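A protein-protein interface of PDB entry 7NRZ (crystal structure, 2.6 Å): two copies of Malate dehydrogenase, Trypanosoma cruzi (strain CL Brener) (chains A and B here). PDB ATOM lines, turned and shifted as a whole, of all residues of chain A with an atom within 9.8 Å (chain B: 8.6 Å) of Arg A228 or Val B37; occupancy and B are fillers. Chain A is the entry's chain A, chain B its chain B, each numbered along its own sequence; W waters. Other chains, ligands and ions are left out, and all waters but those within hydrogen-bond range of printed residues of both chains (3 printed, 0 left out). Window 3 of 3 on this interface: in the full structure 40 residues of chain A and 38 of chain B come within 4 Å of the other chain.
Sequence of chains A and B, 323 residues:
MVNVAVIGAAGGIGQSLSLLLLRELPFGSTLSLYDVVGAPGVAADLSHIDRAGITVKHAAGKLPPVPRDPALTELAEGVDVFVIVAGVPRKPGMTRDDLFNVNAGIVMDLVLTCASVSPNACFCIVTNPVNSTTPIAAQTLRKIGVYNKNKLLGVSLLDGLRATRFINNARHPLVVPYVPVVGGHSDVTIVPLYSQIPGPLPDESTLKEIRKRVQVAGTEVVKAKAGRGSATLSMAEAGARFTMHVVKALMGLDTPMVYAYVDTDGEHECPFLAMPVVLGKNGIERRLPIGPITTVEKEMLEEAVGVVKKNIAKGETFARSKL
O of Ala B10 sits at hydrogen-bond distance from NE2 of Gln B15. The backbone carbonyl oxygen of Ala B9 is in hydrogen-bond range of the backbone NH of Gln B15, at 3.1 Å.
Of the 20 printed residues of chain B, 4 touch a printed residue of chain A. Printed residues of chain B that touch a printed residue of chain A: Gln B15, Val B37, Pro B40 and Gly B41. Hydrophobic or aromatic side chains of chain B that line the printed part of chain A: Val B37 and Pro B40. Of the 17 printed residues of chain A, 4 touch a printed residue of chain B. Printed residues of chain A that touch a printed residue of chain B: Ala A224, Lys A225, Arg A228 and Thr A232. Along chain A the printed residues that touch a printed residue of chain B span positions 224 to 232. Among the printed residues, 5 pairs touch across the chains. Among the printed residues, no Asp or Glu carboxylate lies within 4 Å of a Lys or Arg side-chain nitrogen of the other chain.
Ala A224 touches Pro B40. Lys A225 touches Gly B41. Arg A228 touches Val B37. Thr A232 touches Gln B15 (OG1 to OE1, 3.99 Å).
Arg A228 touches one residue of chain B. Val B37 touches just one residue of chain A: Arg A228 (3.8 Å). No residue of chain B comes within 4 Å of Ala A226. No residue of chain B comes within 4 Å of Gly A227. Val B36 touches none of the printed residues of chain A. No residue of chain A comes within 4 Å of Gly B38. Of the printed residues of chain A, Gly B41 touches Ala A224 (3.3 Å) and Lys A225 (3.6 Å). Printed residues of chain A within 4 Å of Gln B15: Thr A232. Printed residues of chain B within 4 Å of Thr A232: Gln B15 (3.99 Å). Of the printed residues of chain B, Ala A224 touches Pro B40 (3.9 Å) and Gly B41 (3.3 Å). Of the printed residues of chain B, Lys A225 touches Gly B41 (3.6 Å). The nearest residue of chain B that does not touch Arg A228 is Gly B38 (4.03 Å).
Water W1 lies within hydrogen-bond range of O of Ala A224 (2.7 Å), N of Gly B41 (2.8 Å) and O of Gly B38 (3.4 Å). Water W2 lies within hydrogen-bond range of the guanidinium group of Arg A228 (2.8 Å) and the backbone NH of Gly B38 (3.1 Å). Water W3 bridges NZ of Lys A225 and NE2 of Gln B15.
The backbone NH (N) of Gly B41 sits at hydrogen-bond distance from the backbone carbonyl oxygen (O) of Ala A224, 3.3 Å away.
No position is printed for both chains. Of the 5 pairs that touch across the chains among the printed residues, none has its exchanged pair printed and touching as well.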
ATOM      1  N   PRO A  89     -35.992 -11.831  -7.756  1.00  0.00           N
ATOM      2  CA  PRO A  89     -35.226 -10.815  -8.485  1.00  0.00           C
ATOM      3  C   PRO A  89     -35.889 -10.482  -9.812  1.00  0.00           C
ATOM      4  O   PRO A  89     -36.580 -11.310 -10.411  1.00  0.00           O
ATOM      5  CB  PRO A  89     -33.861 -11.481  -8.712  1.00  0.00           C
ATOM      6  CG  PRO A  89     -33.860 -12.727  -7.889  1.00  0.00           C
ATOM      7  CD  PRO A  89     -35.288 -13.121  -7.711  1.00  0.00           C
ATOM      8  N   ARG A  90     -35.660  -9.262 -10.292  1.00  0.00           N
ATOM      9  CA  ARG A  90     -36.234  -8.859 -11.573  1.00  0.00           C
ATOM     10  C   ARG A  90     -35.272  -9.246 -12.687  1.00  0.00           C
ATOM     11  O   ARG A  90     -34.201  -8.649 -12.830  1.00  0.00           O
ATOM     12  CB  ARG A  90     -36.548  -7.367 -11.592  1.00  0.00           C
ATOM     13  CG  ARG A  90     -36.779  -6.797 -12.984  1.00  0.00           C
ATOM     14  CD  ARG A  90     -37.422  -5.422 -12.930  1.00  0.00           C
ATOM     15  NE  ARG A  90     -38.257  -5.153 -14.102  1.00  0.00           N
ATOM     16  CZ  ARG A  90     -38.158  -4.049 -14.837  1.00  0.00           C
ATOM     17  NH1 ARG A  90     -37.267  -3.124 -14.514  1.00  0.00           N
ATOM     18  NH2 ARG A  90     -38.938  -3.864 -15.895  1.00  0.00           N
ATOM     19  N   LYS A  91     -35.632 -10.236 -13.434  1.00  0.00           N
ATOM     20  CA  LYS A  91     -34.932 -10.786 -14.577  1.00  0.00           C
ATOM     21  C   LYS A  91     -35.220  -9.950 -15.820  1.00  0.00           C
ATOM     22  O   LYS A  91     -36.266  -9.300 -15.908  1.00  0.00           O
ATOM     23  CB  LYS A  91     -35.368 -12.229 -14.819  1.00  0.00           C
ATOM     24  CG  LYS A  91     -35.437 -13.079 -13.565  1.00  0.00           C
ATOM     25  CD  LYS A  91     -36.041 -14.443 -13.854  1.00  0.00           C
ATOM     26  CE  LYS A  91     -37.514 -14.496 -13.486  1.00  0.00           C
ATOM     27  NZ  LYS A  91     -38.326 -15.107 -14.571  1.00  0.00           N
ATOM     28  N   PRO A  92     -34.292  -9.935 -16.776  1.00  0.00           N
ATOM     29  CA  PRO A  92     -34.552  -9.242 -18.045  1.00  0.00           C
ATOM     30  C   PRO A  92     -35.793  -9.794 -18.734  1.00  0.00           C
ATOM     31  O   PRO A  92     -35.957 -11.007 -18.881  1.00  0.00           O
ATOM     32  CB  PRO A  92     -33.284  -9.522 -18.858  1.00  0.00           C
ATOM     33  CG  PRO A  92     -32.219  -9.698 -17.824  1.00  0.00           C
ATOM     34  CD  PRO A  92     -32.890 -10.378 -16.663  1.00  0.00           C
ATOM     35  N   THR A 219     -30.028   1.969  -5.128  1.00  0.00           N
ATOM     36  CA  THR A 219     -29.525   1.933  -6.494  1.00  0.00           C
ATOM     37  C   THR A 219     -28.018   2.175  -6.550  1.00  0.00           C
ATOM     38  O   THR A 219     -27.361   1.773  -7.519  1.00  0.00           O
ATOM     39  CB  THR A 219     -30.250   2.968  -7.350  1.00  0.00           C
ATOM     40  OG1 THR A 219     -29.569   4.229  -7.248  1.00  0.00           O
ATOM     41  CG2 THR A 219     -31.690   3.146  -6.899  1.00  0.00           C
ATOM     42  N   VAL A 221     -25.951   0.651  -4.749  1.00  0.00           N
ATOM     43  CA  VAL A 221     -25.385  -0.691  -4.697  1.00  0.00           C
ATOM     44  C   VAL A 221     -25.661  -1.442  -5.993  1.00  0.00           C
ATOM     45  O   VAL A 221     -24.782  -2.134  -6.518  1.00  0.00           O
ATOM     46  CB  VAL A 221     -25.932  -1.441  -3.467  1.00  0.00           C
ATOM     47  CG1 VAL A 221     -25.401  -2.862  -3.423  1.00  0.00           C
ATOM     48  CG2 VAL A 221     -25.563  -0.699  -2.192  1.00  0.00           C
ATOM     49  N   VAL A 222     -26.878  -1.313  -6.531  1.00  0.00           N
ATOM     50  CA  VAL A 222     -27.186  -1.907  -7.831  1.00  0.00           C
ATOM     51  C   VAL A 222     -26.225  -1.388  -8.895  1.00  0.00           C
ATOM     52  O   VAL A 222     -25.725  -2.157  -9.726  1.00  0.00           O
ATOM     53  CB  VAL A 222     -28.657  -1.640  -8.209  1.00  0.00           C
ATOM     54  CG1 VAL A 222     -28.954  -2.157  -9.615  1.00  0.00           C
ATOM     55  CG2 VAL A 222     -29.595  -2.284  -7.193  1.00  0.00           C
ATOM     56  N   LYS A 223     -25.940  -0.083  -8.882  1.00  0.00           N
ATOM     57  CA  LYS A 223     -24.956   0.472  -9.808  1.00  0.00           C
ATOM     58  C   LYS A 223     -23.592  -0.175  -9.604  1.00  0.00           C
ATOM     59  O   LYS A 223     -22.963  -0.644 -10.560  1.00  0.00           O
ATOM     60  CB  LYS A 223     -24.856   1.988  -9.631  1.00  0.00           C
ATOM     61  CG  LYS A 223     -25.489   2.802 -10.754  1.00  0.00           C
ATOM     62  CD  LYS A 223     -26.992   2.580 -10.829  1.00  0.00           C
ATOM     63  CE  LYS A 223     -27.633   3.452 -11.898  1.00  0.00           C
ATOM     64  NZ  LYS A 223     -27.500   4.904 -11.590  1.00  0.00           N
ATOM     65  N   ALA A 224     -23.121  -0.217  -8.352  1.00  0.00           N
ATOM     66  CA  ALA A 224     -21.823  -0.808  -8.049  1.00  0.00           C
ATOM     67  C   ALA A 224     -21.777  -2.300  -8.350  1.00  0.00           C
ATOM     68  O   ALA A 224     -20.682  -2.859  -8.474  1.00  0.00           O
ATOM     69  CB  ALA A 224     -21.460  -0.561  -6.585  1.00  0.00           C
ATOM     70  N   LYS A 225     -22.931  -2.958  -8.463  1.00  0.00           N
ATOM     71  CA  LYS A 225     -22.994  -4.354  -8.871  1.00  0.00           C
ATOM     72  C   LYS A 225     -23.251  -4.507 -10.365  1.00  0.00           C
ATOM     73  O   LYS A 225     -23.616  -5.599 -10.814  1.00  0.00           O
ATOM     74  CB  LYS A 225     -24.061  -5.099  -8.066  1.00  0.00           C
ATOM     75  CG  LYS A 225     -23.612  -5.493  -6.667  1.00  0.00           C
ATOM     76  CD  LYS A 225     -24.688  -6.258  -5.922  1.00  0.00           C
ATOM     77  CE  LYS A 225     -24.313  -6.431  -4.459  1.00  0.00           C
ATOM     78  NZ  LYS A 225     -23.523  -7.673  -4.218  1.00  0.00           N
ATOM     79  N   ALA A 226     -23.071  -3.433 -11.139  1.00  0.00           N
ATOM     80  CA  ALA A 226     -23.264  -3.443 -12.592  1.00  0.00           C
ATOM     81  C   ALA A 226     -24.649  -3.964 -12.971  1.00  0.00           C
ATOM     82  O   ALA A 226     -24.834  -4.613 -14.003  1.00  0.00           O
ATOM     83  CB  ALA A 226     -22.170  -4.253 -13.288  1.00  0.00           C
ATOM     84  N   GLY A 227     -25.636  -3.678 -12.124  1.00  0.00           N
ATOM     85  CA  GLY A 227     -26.993  -4.116 -12.374  1.00  0.00           C
ATOM     86  C   GLY A 227     -27.251  -5.594 -12.183  1.00  0.00           C
ATOM     87  O   GLY A 227     -28.361  -6.053 -12.474  1.00  0.00           O
ATOM     88  N   ARG A 228     -26.274  -6.357 -11.698  1.00  0.00           N
ATOM     89  CA  ARG A 228     -26.414  -7.801 -11.571  1.00  0.00           C
ATOM     90  C   ARG A 228     -26.942  -8.237 -10.208  1.00  0.00           C
ATOM     91  O   ARG A 228     -26.943  -9.436  -9.913  1.00  0.00           O
ATOM     92  CB  ARG A 228     -25.073  -8.489 -11.849  1.00  0.00           C
ATOM     93  CG  ARG A 228     -24.356  -7.984 -13.087  1.00  0.00           C
ATOM     94  CD  ARG A 228     -23.043  -8.728 -13.303  1.00  0.00           C
ATOM     95  NE  ARG A 228     -21.891  -7.963 -12.827  1.00  0.00           N
ATOM     96  CZ  ARG A 228     -21.267  -8.177 -11.671  1.00  0.00           C
ATOM     97  NH1 ARG A 228     -21.675  -9.142 -10.854  1.00  0.00           N
ATOM     98  NH2 ARG A 228     -20.228  -7.425 -11.330  1.00  0.00           N
ATOM     99  N   GLY A 229     -27.399  -7.304  -9.384  1.00  0.00           N
ATOM    100  CA  GLY A 229     -27.874  -7.646  -8.060  1.00  0.00           C
ATOM    101  C   GLY A 229     -28.074  -6.395  -7.234  1.00  0.00           C
ATOM    102  O   GLY A 229     -27.877  -5.272  -7.705  1.00  0.00           O
ATOM    103  N   SER A 230     -28.465  -6.614  -5.982  1.00  0.00           N
ATOM    104  CA  SER A 230     -28.786  -5.526  -5.070  1.00  0.00           C
ATOM    105  C   SER A 230     -28.140  -5.791  -3.715  1.00  0.00           C
ATOM    106  O   SER A 230     -27.445  -6.792  -3.516  1.00  0.00           O
ATOM    107  CB  SER A 230     -30.304  -5.353  -4.933  1.00  0.00           C
ATOM    108  OG  SER A 230     -30.935  -6.591  -4.654  1.00  0.00           O
ATOM    109  N   ALA A 231     -28.376  -4.874  -2.778  1.00  0.00           N
ATOM    110  CA  ALA A 231     -27.818  -5.009  -1.439  1.00  0.00           C
ATOM    111  C   ALA A 231     -28.356  -6.266  -0.772  1.00  0.00           C
ATOM    112  O   ALA A 231     -29.568  -6.419  -0.600  1.00  0.00           O
ATOM    113  CB  ALA A 231     -28.150  -3.774  -0.604  1.00  0.00           C
ATOM    114  N   THR A 232     -27.461  -7.176  -0.423  1.00  0.00           N
ATOM    115  CA  THR A 232     -27.846  -8.380   0.298  1.00  0.00           C
ATOM    116  C   THR A 232     -27.213  -8.471   1.674  1.00  0.00           C
ATOM    117  O   THR A 232     -27.901  -8.812   2.642  1.00  0.00           O
ATOM    118  CB  THR A 232     -27.485  -9.635  -0.515  1.00  0.00           C
ATOM    119  OG1 THR A 232     -26.068  -9.703  -0.692  1.00  0.00           O
ATOM    120  CG2 THR A 232     -28.152  -9.595  -1.875  1.00  0.00           C
ATOM    121  N   GLY B   8     -10.717 -12.629  -2.577  1.00  0.00           N
ATOM    122  CA  GLY B   8     -11.809 -13.487  -3.001  1.00  0.00           C
ATOM    123  C   GLY B   8     -13.090 -13.147  -2.265  1.00  0.00           C
ATOM    124  O   GLY B   8     -13.848 -14.038  -1.870  1.00  0.00           O
ATOM    125  N   ALA B   9     -13.347 -11.849  -2.090  1.00  0.00           N
ATOM    126  CA  ALA B   9     -14.403 -11.368  -1.207  1.00  0.00           C
ATOM    127  C   ALA B   9     -15.797 -11.425  -1.817  1.00  0.00           C
ATOM    128  O   ALA B   9     -16.775 -11.233  -1.085  1.00  0.00           O
ATOM    129  CB  ALA B   9     -14.110  -9.928  -0.775  1.00  0.00           C
ATOM    130  N   ALA B  10     -15.922 -11.667  -3.122  1.00  0.00           N
ATOM    131  CA  ALA B  10     -17.219 -11.607  -3.782  1.00  0.00           C
ATOM    132  C   ALA B  10     -17.863 -12.971  -3.988  1.00  0.00           C
ATOM    133  O   ALA B  10     -19.028 -13.030  -4.392  1.00  0.00           O
ATOM    134  CB  ALA B  10     -17.095 -10.899  -5.135  1.00  0.00           C
ATOM    135  N   GLY B  11     -17.146 -14.058  -3.731  1.00  0.00           N
ATOM    136  CA  GLY B  11     -17.731 -15.376  -3.824  1.00  0.00           C
ATOM    137  C   GLY B  11     -18.719 -15.614  -2.697  1.00  0.00           C
ATOM    138  O   GLY B  11     -18.902 -14.797  -1.794  1.00  0.00           O
ATOM    139  N   GLN B  15     -18.253 -13.323   0.683  1.00  0.00           N
ATOM    140  CA  GLN B  15     -19.236 -12.298   1.029  1.00  0.00           C
ATOM    141  C   GLN B  15     -19.680 -12.426   2.484  1.00  0.00           C
ATOM    142  O   GLN B  15     -19.649 -11.449   3.242  1.00  0.00           O
ATOM    143  CB  GLN B  15     -20.437 -12.370   0.083  1.00  0.00           C
ATOM    144  CG  GLN B  15     -20.153 -11.832  -1.312  1.00  0.00           C
ATOM    145  CD  GLN B  15     -21.401 -11.328  -2.021  1.00  0.00           C
ATOM    146  OE1 GLN B  15     -22.280 -10.718  -1.409  1.00  0.00           O
ATOM    147  NE2 GLN B  15     -21.479 -11.577  -3.323  1.00  0.00           N
ATOM    148  N   TYR B  34     -10.879  -7.689  -2.139  1.00  0.00           N
ATOM    149  CA  TYR B  34     -10.407  -7.879  -3.500  1.00  0.00           C
ATOM    150  C   TYR B  34     -11.118  -9.068  -4.114  1.00  0.00           C
ATOM    151  O   TYR B  34     -11.227 -10.131  -3.493  1.00  0.00           O
ATOM    152  CB  TYR B  34      -8.892  -8.098  -3.571  1.00  0.00           C
ATOM    153  CG  TYR B  34      -8.400  -8.389  -4.978  1.00  0.00           C
ATOM    154  CD1 TYR B  34      -8.204  -7.361  -5.895  1.00  0.00           C
ATOM    155  CD2 TYR B  34      -8.141  -9.689  -5.393  1.00  0.00           C
ATOM    156  CE1 TYR B  34      -7.761  -7.624  -7.181  1.00  0.00           C
ATOM    157  CE2 TYR B  34      -7.698  -9.958  -6.673  1.00  0.00           C
ATOM    158  CZ  TYR B  34      -7.510  -8.924  -7.562  1.00  0.00           C
ATOM    159  OH  TYR B  34      -7.068  -9.190  -8.837  1.00  0.00           O
ATOM    160  N   ASP B  35     -11.603  -8.877  -5.331  1.00  0.00           N
ATOM    161  CA  ASP B  35     -12.011  -9.997  -6.153  1.00  0.00           C
ATOM    162  C   ASP B  35     -11.871  -9.586  -7.604  1.00  0.00           C
ATOM    163  O   ASP B  35     -11.755  -8.402  -7.938  1.00  0.00           O
ATOM    164  CB  ASP B  35     -13.439 -10.465  -5.846  1.00  0.00           C
ATOM    165  CG  ASP B  35     -13.637 -11.946  -6.126  1.00  0.00           C
ATOM    166  OD1 ASP B  35     -13.138 -12.428  -7.165  1.00  0.00           O
ATOM    167  OD2 ASP B  35     -14.280 -12.629  -5.300  1.00  0.00           O
ATOM    168  N   VAL B  36     -11.864 -10.602  -8.461  1.00  0.00           N
ATOM    169  CA  VAL B  36     -11.734 -10.408  -9.895  1.00  0.00           C
ATOM    170  C   VAL B  36     -13.062 -10.012 -10.542  1.00  0.00           C
ATOM    171  O   VAL B  36     -13.068  -9.472 -11.657  1.00  0.00           O
ATOM    172  CB  VAL B  36     -11.080 -11.685 -10.453  1.00  0.00           C
ATOM    173  CG1 VAL B  36     -12.108 -12.765 -10.766  1.00  0.00           C
ATOM    174  CG2 VAL B  36     -10.289 -11.344 -11.698  1.00  0.00           C
ATOM    175  N   VAL B  37     -14.180 -10.216  -9.846  1.00  0.00           N
ATOM    176  CA  VAL B  37     -15.483  -9.688 -10.242  1.00  0.00           C
ATOM    177  C   VAL B  37     -16.282  -9.422  -8.972  1.00  0.00           C
ATOM    178  O   VAL B  37     -16.145 -10.143  -7.982  1.00  0.00           O
ATOM    179  CB  VAL B  37     -16.225 -10.660 -11.189  1.00  0.00           C
ATOM    180  CG1 VAL B  37     -16.383 -12.034 -10.542  1.00  0.00           C
ATOM    181  CG2 VAL B  37     -17.577 -10.095 -11.604  1.00  0.00           C
ATOM    182  N   GLY B  38     -17.088  -8.357  -8.988  1.00  0.00           N
ATOM    183  CA  GLY B  38     -18.058  -8.103  -7.938  1.00  0.00           C
ATOM    184  C   GLY B  38     -17.539  -7.448  -6.673  1.00  0.00           C
ATOM    185  O   GLY B  38     -18.328  -7.230  -5.746  1.00  0.00           O
ATOM    186  N   ALA B  39     -16.248  -7.129  -6.602  1.00  0.00           N
ATOM    187  CA  ALA B  39     -15.703  -6.492  -5.405  1.00  0.00           C
ATOM    188  C   ALA B  39     -16.314  -5.123  -5.122  1.00  0.00           C
ATOM    189  O   ALA B  39     -16.703  -4.876  -3.968  1.00  0.00           O
ATOM    190  CB  ALA B  39     -14.175  -6.412  -5.517  1.00  0.00           C
ATOM    191  N   PRO B  40     -16.425  -4.196  -6.086  1.00  0.00           N
ATOM    192  CA  PRO B  40     -17.045  -2.899  -5.756  1.00  0.00           C
ATOM    193  C   PRO B  40     -18.453  -3.024  -5.195  1.00  0.00           C
ATOM    194  O   PRO B  40     -18.830  -2.255  -4.303  1.00  0.00           O
ATOM    195  CB  PRO B  40     -17.026  -2.154  -7.101  1.00  0.00           C
ATOM    196  CG  PRO B  40     -15.924  -2.783  -7.866  1.00  0.00           C
ATOM    197  CD  PRO B  40     -15.940  -4.225  -7.480  1.00  0.00           C
ATOM    198  N   GLY B  41     -19.239  -3.982  -5.691  1.00  0.00           N
ATOM    199  CA  GLY B  41     -20.595  -4.143  -5.195  1.00  0.00           C
ATOM    200  C   GLY B  41     -20.641  -4.679  -3.777  1.00  0.00           C
ATOM    201  O   GLY B  41     -21.460  -4.239  -2.965  1.00  0.00           O
ATOM    202  N   VAL B  42     -19.770  -5.641  -3.459  1.00  0.00           N
ATOM    203  CA  VAL B  42     -19.686  -6.128  -2.084  1.00  0.00           C
ATOM    204  C   VAL B  42     -19.259  -5.001  -1.155  1.00  0.00           C
ATOM    205  O   VAL B  42     -19.838  -4.809  -0.078  1.00  0.00           O
ATOM    206  CB  VAL B  42     -18.730  -7.332  -1.991  1.00  0.00           C
ATOM    207  CG1 VAL B  42     -18.508  -7.722  -0.535  1.00  0.00           C
ATOM    208  CG2 VAL B  42     -19.277  -8.508  -2.785  1.00  0.00           C
ATOM    209  N   ALA B  59     -10.759  -3.227  -4.354  1.00  0.00           N
ATOM    210  CA  ALA B  59     -10.061  -3.159  -5.627  1.00  0.00           C
ATOM    211  C   ALA B  59     -10.603  -4.263  -6.519  1.00  0.00           C
ATOM    212  O   ALA B  59     -10.822  -5.386  -6.059  1.00  0.00           O
ATOM    213  CB  ALA B  59      -8.544  -3.302  -5.457  1.00  0.00           C
ATOM    214  N   ALA B  60     -10.828  -3.934  -7.788  1.00  0.00           N
ATOM    215  CA  ALA B  60     -11.359  -4.873  -8.768  1.00  0.00           C
ATOM    216  C   ALA B  60     -10.233  -5.307  -9.694  1.00  0.00           C
ATOM    217  O   ALA B  60      -9.631  -4.471 -10.377  1.00  0.00           O
ATOM    218  CB  ALA B  60     -12.498  -4.247  -9.569  1.00  0.00           C
ATOM    219  N   GLY B  61     -10.009  -6.623  -9.778  1.00  0.00           N
ATOM    220  CA  GLY B  61      -8.992  -7.152 -10.708  1.00  0.00           C
ATOM    221  C   GLY B  61      -9.562  -7.340 -12.103  1.00  0.00           C
ATOM    222  O   GLY B  61     -10.801  -7.390 -12.228  1.00  0.00           O
ATOM    223  N   LYS B  62      -8.692  -7.511 -13.072  1.00  0.00           N
ATOM    224  CA  LYS B  62      -9.165  -7.613 -14.451  1.00  0.00           C
ATOM    225  C   LYS B  62      -9.754  -8.987 -14.678  1.00  0.00           C
ATOM    226  O   LYS B  62      -9.162  -9.945 -14.228  1.00  0.00           O
ATOM    227  CB  LYS B  62      -8.007  -7.277 -15.384  1.00  0.00           C
ATOM    228  N   LEU B  63     -10.911  -9.038 -15.311  1.00  0.00           N
ATOM    229  CA  LEU B  63     -11.532 -10.319 -15.709  1.00  0.00           C
ATOM    230  C   LEU B  63     -11.491 -10.285 -17.233  1.00  0.00           C
ATOM    231  O   LEU B  63     -11.964  -9.290 -17.779  1.00  0.00           O
ATOM    232  CB  LEU B  63     -12.980 -10.318 -15.221  1.00  0.00           C
ATOM    233  CG  LEU B  63     -13.742 -11.631 -15.351  1.00  0.00           C
ATOM    234  CD1 LEU B  63     -13.179 -12.676 -14.409  1.00  0.00           C
ATOM    235  CD2 LEU B  63     -15.216 -11.414 -15.068  1.00  0.00           C
ATOM    236  N   PRO B  65      -8.896 -13.151 -15.565  1.00  0.00           N
ATOM    237  CA  PRO B  65      -7.724 -13.032 -14.715  1.00  0.00           C
ATOM    238  C   PRO B  65      -6.327 -12.713 -15.260  1.00  0.00           C
ATOM    239  O   PRO B  65      -5.851 -13.423 -16.100  1.00  0.00           O
ATOM    240  CB  PRO B  65      -7.791 -14.363 -13.971  1.00  0.00           C
ATOM    241  CG  PRO B  65      -9.253 -14.587 -13.776  1.00  0.00           C
ATOM    242  CD  PRO B  65      -9.820 -14.186 -15.114  1.00  0.00           C
HETATM  243  O   HOH W   1     -19.300  -5.206  -8.260  1.00  0.00           O
HETATM  244  O   HOH W   2     -17.686  -6.243 -11.164  1.00  0.00           O
HETATM  245  O   HOH W   3     -23.831 -10.321  -5.144  1.00  0.00           O
